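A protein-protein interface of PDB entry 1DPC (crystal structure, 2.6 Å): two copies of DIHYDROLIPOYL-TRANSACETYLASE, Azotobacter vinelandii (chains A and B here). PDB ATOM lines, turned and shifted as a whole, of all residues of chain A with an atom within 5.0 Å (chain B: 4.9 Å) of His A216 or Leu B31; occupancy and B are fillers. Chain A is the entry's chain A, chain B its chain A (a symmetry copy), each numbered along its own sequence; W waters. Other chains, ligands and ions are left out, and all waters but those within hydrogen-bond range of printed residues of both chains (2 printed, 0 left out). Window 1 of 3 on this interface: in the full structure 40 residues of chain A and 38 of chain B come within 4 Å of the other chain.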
ATOM      1  N   PRO A  39      19.778  -2.732  18.302  1.00  0.00           N
ATOM      2  CA  PRO A  39      18.884  -3.726  17.756  1.00  0.00           C
ATOM      3  C   PRO A  39      17.480  -3.150  17.802  1.00  0.00           C
ATOM      4  O   PRO A  39      16.928  -2.976  18.898  1.00  0.00           O
ATOM      5  CB  PRO A  39      19.152  -4.921  18.628  1.00  0.00           C
ATOM      6  CG  PRO A  39      19.683  -4.371  19.901  1.00  0.00           C
ATOM      7  CD  PRO A  39      20.551  -3.258  19.419  1.00  0.00           C
ATOM      8  N   VAL A  41      13.377  -2.630  17.044  1.00  0.00           N
ATOM      9  CA  VAL A  41      12.067  -3.261  16.865  1.00  0.00           C
ATOM     10  C   VAL A  41      11.088  -2.116  16.712  1.00  0.00           C
ATOM     11  O   VAL A  41      11.284  -1.080  17.344  1.00  0.00           O
ATOM     12  CB  VAL A  41      11.629  -4.126  18.076  1.00  0.00           C
ATOM     13  CG1 VAL A  41      10.248  -4.754  17.855  1.00  0.00           C
ATOM     14  CG2 VAL A  41      12.603  -5.266  18.241  1.00  0.00           C
ATOM     15  N   TYR A 214      12.207   0.995  19.079  1.00  0.00           N
ATOM     16  CA  TYR A 214      12.908   1.107  20.338  1.00  0.00           C
ATOM     17  C   TYR A 214      14.157   0.290  20.361  1.00  0.00           C
ATOM     18  O   TYR A 214      14.367  -0.568  19.498  1.00  0.00           O
ATOM     19  CB  TYR A 214      11.991   0.684  21.457  1.00  0.00           C
ATOM     20  CG  TYR A 214      11.322  -0.663  21.291  1.00  0.00           C
ATOM     21  CD1 TYR A 214      11.952  -1.800  21.794  1.00  0.00           C
ATOM     22  CD2 TYR A 214      10.060  -0.757  20.693  1.00  0.00           C
ATOM     23  CE1 TYR A 214      11.323  -3.047  21.712  1.00  0.00           C
ATOM     24  CE2 TYR A 214       9.433  -2.007  20.603  1.00  0.00           C
ATOM     25  CZ  TYR A 214      10.072  -3.136  21.118  1.00  0.00           C
ATOM     26  OH  TYR A 214       9.460  -4.361  21.071  1.00  0.00           O
ATOM     27  N   ASP A 215      14.992   0.615  21.328  1.00  0.00           N
ATOM     28  CA  ASP A 215      16.247  -0.065  21.517  1.00  0.00           C
ATOM     29  C   ASP A 215      15.909  -1.295  22.327  1.00  0.00           C
ATOM     30  O   ASP A 215      15.762  -1.225  23.550  1.00  0.00           O
ATOM     31  CB  ASP A 215      17.198   0.796  22.297  1.00  0.00           C
ATOM     32  CG  ASP A 215      18.599   0.231  22.453  1.00  0.00           C
ATOM     33  OD1 ASP A 215      18.816  -0.978  22.415  1.00  0.00           O
ATOM     34  OD2 ASP A 215      19.497   1.039  22.612  1.00  0.00           O
ATOM     35  N   HIS A 216      15.923  -2.443  21.669  1.00  0.00           N
ATOM     36  CA  HIS A 216      15.495  -3.653  22.331  1.00  0.00           C
ATOM     37  C   HIS A 216      16.427  -4.138  23.429  1.00  0.00           C
ATOM     38  O   HIS A 216      16.067  -5.053  24.170  1.00  0.00           O
ATOM     39  CB  HIS A 216      15.297  -4.745  21.289  1.00  0.00           C
ATOM     40  CG  HIS A 216      14.405  -5.881  21.792  1.00  0.00           C
ATOM     41  ND1 HIS A 216      13.861  -6.080  22.990  1.00  0.00           N
ATOM     42  CD2 HIS A 216      14.026  -6.942  21.013  1.00  0.00           C
ATOM     43  CE1 HIS A 216      13.187  -7.196  22.961  1.00  0.00           C
ATOM     44  NE2 HIS A 216      13.292  -7.708  21.768  1.00  0.00           N
ATOM     45  N   ARG A 217      17.626  -3.577  23.556  1.00  0.00           N
ATOM     46  CA  ARG A 217      18.532  -3.903  24.663  1.00  0.00           C
ATOM     47  C   ARG A 217      18.043  -3.367  25.995  1.00  0.00           C
ATOM     48  O   ARG A 217      18.303  -3.918  27.055  1.00  0.00           O
ATOM     49  CB  ARG A 217      19.920  -3.306  24.484  1.00  0.00           C
ATOM     50  CG  ARG A 217      20.584  -3.842  23.227  1.00  0.00           C
ATOM     51  CD  ARG A 217      21.872  -3.134  22.968  1.00  0.00           C
ATOM     52  NE  ARG A 217      21.618  -1.726  22.854  1.00  0.00           N
ATOM     53  CZ  ARG A 217      22.588  -0.883  22.563  1.00  0.00           C
ATOM     54  NH1 ARG A 217      23.836  -1.308  22.362  1.00  0.00           N
ATOM     55  NH2 ARG A 217      22.305   0.411  22.504  1.00  0.00           N
ATOM     56  N   VAL A 218      17.364  -2.237  25.895  1.00  0.00           N
ATOM     57  CA  VAL A 218      16.884  -1.513  27.038  1.00  0.00           C
ATOM     58  C   VAL A 218      15.386  -1.768  27.175  1.00  0.00           C
ATOM     59  O   VAL A 218      14.908  -1.994  28.287  1.00  0.00           O
ATOM     60  CB  VAL A 218      17.242  -0.042  26.774  1.00  0.00           C
ATOM     61  CG1 VAL A 218      16.668   0.842  27.862  1.00  0.00           C
ATOM     62  CG2 VAL A 218      18.758   0.111  26.687  1.00  0.00           C
ATOM     63  N   ILE A 219      14.598  -1.739  26.097  1.00  0.00           N
ATOM     64  CA  ILE A 219      13.167  -1.971  26.185  1.00  0.00           C
ATOM     65  C   ILE A 219      12.755  -3.303  25.591  1.00  0.00           C
ATOM     66  O   ILE A 219      13.141  -3.670  24.473  1.00  0.00           O
ATOM     67  CB  ILE A 219      12.464  -0.798  25.488  1.00  0.00           C
ATOM     68  CG1 ILE A 219      12.535   0.367  26.426  1.00  0.00           C
ATOM     69  CG2 ILE A 219      10.998  -1.060  25.203  1.00  0.00           C
ATOM     70  CD1 ILE A 219      12.939   1.497  25.543  1.00  0.00           C
ATOM     71  N   ASP A 220      12.001  -4.086  26.347  1.00  0.00           N
ATOM     72  CA  ASP A 220      11.495  -5.360  25.854  1.00  0.00           C
ATOM     73  C   ASP A 220      10.132  -5.162  25.221  1.00  0.00           C
ATOM     74  O   ASP A 220       9.433  -4.172  25.438  1.00  0.00           O
ATOM     75  CB  ASP A 220      11.370  -6.381  26.994  1.00  0.00           C
ATOM     76  CG  ASP A 220      10.421  -5.937  28.119  1.00  0.00           C
ATOM     77  OD1 ASP A 220       9.210  -6.156  28.010  1.00  0.00           O
ATOM     78  OD2 ASP A 220      10.891  -5.368  29.107  1.00  0.00           O
ATOM     79  N   GLY A 221       9.687  -6.205  24.559  1.00  0.00           N
ATOM     80  CA  GLY A 221       8.458  -6.164  23.814  1.00  0.00           C
ATOM     81  C   GLY A 221       7.250  -5.765  24.616  1.00  0.00           C
ATOM     82  O   GLY A 221       6.497  -4.880  24.204  1.00  0.00           O
ATOM     83  N   GLY B  27      20.853 -10.660  27.635  1.00  0.00           N
ATOM     84  CA  GLY B  27      19.856 -10.407  26.621  1.00  0.00           C
ATOM     85  C   GLY B  27      20.361  -9.366  25.642  1.00  0.00           C
ATOM     86  O   GLY B  27      20.353  -9.641  24.442  1.00  0.00           O
ATOM     87  N   ALA B  28      20.933  -8.272  26.153  1.00  0.00           N
ATOM     88  CA  ALA B  28      21.384  -7.184  25.323  1.00  0.00           C
ATOM     89  C   ALA B  28      22.403  -7.694  24.345  1.00  0.00           C
ATOM     90  O   ALA B  28      22.272  -7.536  23.132  1.00  0.00           O
ATOM     91  CB  ALA B  28      22.014  -6.121  26.167  1.00  0.00           C
ATOM     92  N   THR B  29      23.358  -8.437  24.858  1.00  0.00           N
ATOM     93  CA  THR B  29      24.432  -8.971  24.041  1.00  0.00           C
ATOM     94  C   THR B  29      23.960  -9.885  22.931  1.00  0.00           C
ATOM     95  O   THR B  29      24.391  -9.778  21.775  1.00  0.00           O
ATOM     96  CB  THR B  29      25.358  -9.668  25.016  1.00  0.00           C
ATOM     97  OG1 THR B  29      25.794  -8.631  25.887  1.00  0.00           O
ATOM     98  CG2 THR B  29      26.503 -10.409  24.369  1.00  0.00           C
ATOM     99  N   ASN B  30      23.018 -10.747  23.280  1.00  0.00           N
ATOM    100  CA  ASN B  30      22.536 -11.692  22.304  1.00  0.00           C
ATOM    101  C   ASN B  30      21.735 -11.019  21.219  1.00  0.00           C
ATOM    102  O   ASN B  30      21.881 -11.349  20.031  1.00  0.00           O
ATOM    103  CB  ASN B  30      21.664 -12.749  22.948  1.00  0.00           C
ATOM    104  CG  ASN B  30      22.517 -13.694  23.763  1.00  0.00           C
ATOM    105  OD1 ASN B  30      23.481 -14.298  23.291  1.00  0.00           O
ATOM    106  ND2 ASN B  30      22.239 -13.827  25.043  1.00  0.00           N
ATOM    107  N   LEU B  31      20.914 -10.020  21.581  1.00  0.00           N
ATOM    108  CA  LEU B  31      20.114  -9.321  20.590  1.00  0.00           C
ATOM    109  C   LEU B  31      20.992  -8.568  19.611  1.00  0.00           C
ATOM    110  O   LEU B  31      20.741  -8.570  18.399  1.00  0.00           O
ATOM    111  CB  LEU B  31      19.187  -8.335  21.257  1.00  0.00           C
ATOM    112  CG  LEU B  31      18.093  -8.935  22.099  1.00  0.00           C
ATOM    113  CD1 LEU B  31      17.469  -7.810  22.874  1.00  0.00           C
ATOM    114  CD2 LEU B  31      17.067  -9.657  21.248  1.00  0.00           C
ATOM    115  N   HIS B  32      22.047  -7.935  20.129  1.00  0.00           N
ATOM    116  CA  HIS B  32      22.914  -7.211  19.257  1.00  0.00           C
ATOM    117  C   HIS B  32      23.651  -8.163  18.315  1.00  0.00           C
ATOM    118  O   HIS B  32      23.826  -7.855  17.134  1.00  0.00           O
ATOM    119  CB  HIS B  32      23.852  -6.413  20.116  1.00  0.00           C
ATOM    120  CG  HIS B  32      24.432  -5.222  19.360  1.00  0.00           C
ATOM    121  ND1 HIS B  32      25.567  -4.592  19.609  1.00  0.00           N
ATOM    122  CD2 HIS B  32      23.862  -4.611  18.263  1.00  0.00           C
ATOM    123  CE1 HIS B  32      25.714  -3.646  18.719  1.00  0.00           C
ATOM    124  NE2 HIS B  32      24.685  -3.669  17.914  1.00  0.00           N
ATOM    125  N   ARG B  33      24.023  -9.349  18.780  1.00  0.00           N
ATOM    126  CA  ARG B  33      24.701 -10.356  17.975  1.00  0.00           C
ATOM    127  C   ARG B  33      23.793 -10.777  16.796  1.00  0.00           C
ATOM    128  O   ARG B  33      24.162 -10.724  15.617  1.00  0.00           O
ATOM    129  CB  ARG B  33      25.019 -11.482  18.961  1.00  0.00           C
ATOM    130  CG  ARG B  33      26.296 -12.249  18.787  1.00  0.00           C
ATOM    131  CD  ARG B  33      26.030 -13.697  19.153  1.00  0.00           C
ATOM    132  NE  ARG B  33      25.741 -13.937  20.556  1.00  0.00           N
ATOM    133  CZ  ARG B  33      26.725 -14.005  21.454  1.00  0.00           C
ATOM    134  NH1 ARG B  33      28.007 -13.851  21.093  1.00  0.00           N
ATOM    135  NH2 ARG B  33      26.422 -14.282  22.718  1.00  0.00           N
ATOM    136  N   SER B  34      22.534 -11.116  17.092  1.00  0.00           N
ATOM    137  CA  SER B  34      21.556 -11.443  16.071  1.00  0.00           C
ATOM    138  C   SER B  34      21.374 -10.314  15.100  1.00  0.00           C
ATOM    139  O   SER B  34      21.417 -10.525  13.898  1.00  0.00           O
ATOM    140  CB  SER B  34      20.205 -11.701  16.648  1.00  0.00           C
ATOM    141  OG  SER B  34      20.130 -12.896  17.404  1.00  0.00           O
ATOM    142  N   TRP B  35      21.207  -9.098  15.609  1.00  0.00           N
ATOM    143  CA  TRP B  35      20.933  -7.926  14.809  1.00  0.00           C
ATOM    144  C   TRP B  35      22.010  -7.726  13.772  1.00  0.00           C
ATOM    145  O   TRP B  35      21.688  -7.531  12.603  1.00  0.00           O
ATOM    146  CB  TRP B  35      20.839  -6.706  15.726  1.00  0.00           C
ATOM    147  CG  TRP B  35      20.527  -5.396  15.016  1.00  0.00           C
ATOM    148  CD1 TRP B  35      21.459  -4.387  14.911  1.00  0.00           C
ATOM    149  CD2 TRP B  35      19.336  -5.089  14.406  1.00  0.00           C
ATOM    150  NE1 TRP B  35      20.853  -3.434  14.224  1.00  0.00           N
ATOM    151  CE2 TRP B  35      19.599  -3.802  13.911  1.00  0.00           C
ATOM    152  CE3 TRP B  35      18.096  -5.701  14.214  1.00  0.00           C
ATOM    153  CZ2 TRP B  35      18.620  -3.118  13.207  1.00  0.00           C
ATOM    154  CZ3 TRP B  35      17.118  -5.011  13.518  1.00  0.00           C
ATOM    155  CH2 TRP B  35      17.381  -3.731  13.011  1.00  0.00           C
ATOM    156  N   ILE B 177      12.946  -9.662  16.686  1.00  0.00           N
ATOM    157  CA  ILE B 177      14.285 -10.029  16.278  1.00  0.00           C
ATOM    158  C   ILE B 177      14.440 -11.536  16.463  1.00  0.00           C
ATOM    159  O   ILE B 177      13.962 -12.166  17.396  1.00  0.00           O
ATOM    160  CB  ILE B 177      15.313  -9.222  17.121  1.00  0.00           C
ATOM    161  CG1 ILE B 177      15.325  -7.780  16.636  1.00  0.00           C
ATOM    162  CG2 ILE B 177      16.715  -9.775  16.966  1.00  0.00           C
ATOM    163  CD1 ILE B 177      16.130  -6.883  17.574  1.00  0.00           C
ATOM    164  N   ASN B 179      16.070 -14.980  17.001  1.00  0.00           N
ATOM    165  CA  ASN B 179      17.000 -15.450  18.002  1.00  0.00           C
ATOM    166  C   ASN B 179      17.958 -16.390  17.292  1.00  0.00           C
ATOM    167  O   ASN B 179      17.747 -17.605  17.210  1.00  0.00           O
ATOM    168  CB  ASN B 179      16.301 -16.206  19.104  1.00  0.00           C
ATOM    169  CG  ASN B 179      15.329 -15.332  19.857  1.00  0.00           C
ATOM    170  OD1 ASN B 179      15.609 -14.191  20.240  1.00  0.00           O
ATOM    171  ND2 ASN B 179      14.130 -15.861  20.046  1.00  0.00           N
HETATM  172  O   HOH W   1      18.161  -7.057  27.762  1.00  0.00           O
HETATM  173  O   HOH W   2      12.003  -9.508  19.403  1.00  0.00           O
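Hydrophobic or aromatic side chains of chain B that line the printed part of chain A: Ala B28, Leu B31, His B32, Trp B35 and Ile B177. Among the printed residues, 7 pairs touch across the chains. Among the printed residues, no Asp or Glu carboxylate lies within 4 Å of a Lys or Arg side-chain nitrogen of the other chain.
Of chain B, only Leu B31 (3.4 Å) comes within 4 Å of His A216. Printed residues of chain A within 4 Å of Leu B31: Pro A39 (3.99 Å) and His A216 (3.4 Å). Printed residues of chain A within 4 Å of Trp B35: Pro A39. Of the printed residues of chain A, Ala B28 touches Arg A217. Of the printed residues of chain A, Ile B177 touches Pro A39 and Val A41. Printed residues of chain B within 4 Å of Arg A217: Ala B28. Thr B29 touches none of the printed residues of chain A. Asn B179 touches none of the printed residues of chain A. The nearest residue of chain B that does not touch His A216 is Ile B177 (4.03 Å). The nearest printed residue of chain A that does not touch Leu B31 is Arg A217 (4.3 Å).
No position is printed for both chains. Of the 7 pairs that touch across the chains among the printed residues, none has its exchanged pair printed and touching as well.
Among the printed residues, pairs that only touch across the chains: His A216 with Leu B31 (3.4 Å), Pro A39 with Trp B35 (3.6 Å), Pro A39 with Ile B177 (3.8 Å), Pro A39 with His B32 (3.8 Å), Arg A217 with Ala B28 (3.9 Å), Val A41 with Ile B177 (3.9 Å) and Pro A39 with Leu B31 (3.99 Å).
Water W2 bridges N of Ile B177 (2.9 Å) and NE2 of His A216 (3.2 Å). Water W1 lies within hydrogen-bond range of O of Arg A217 (3.2 Å) and N of Ala B28 (3.4 Å).
The guanidinium group of Arg A217 lies within salt-bridge range of the side-chain carboxylate of Asp A215, at 2.9 Å. ND1 of His A216 sits at hydrogen-bond distance from O of Ile A219 (2.9 Å). The backbone carbonyl oxygen of Pro A39 is in hydrogen-bond range of the backbone NH of His A216, at 3.0 Å. N of Tyr A214 is in hydrogen-bond range of O of Val A41, 2.9 Å away.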
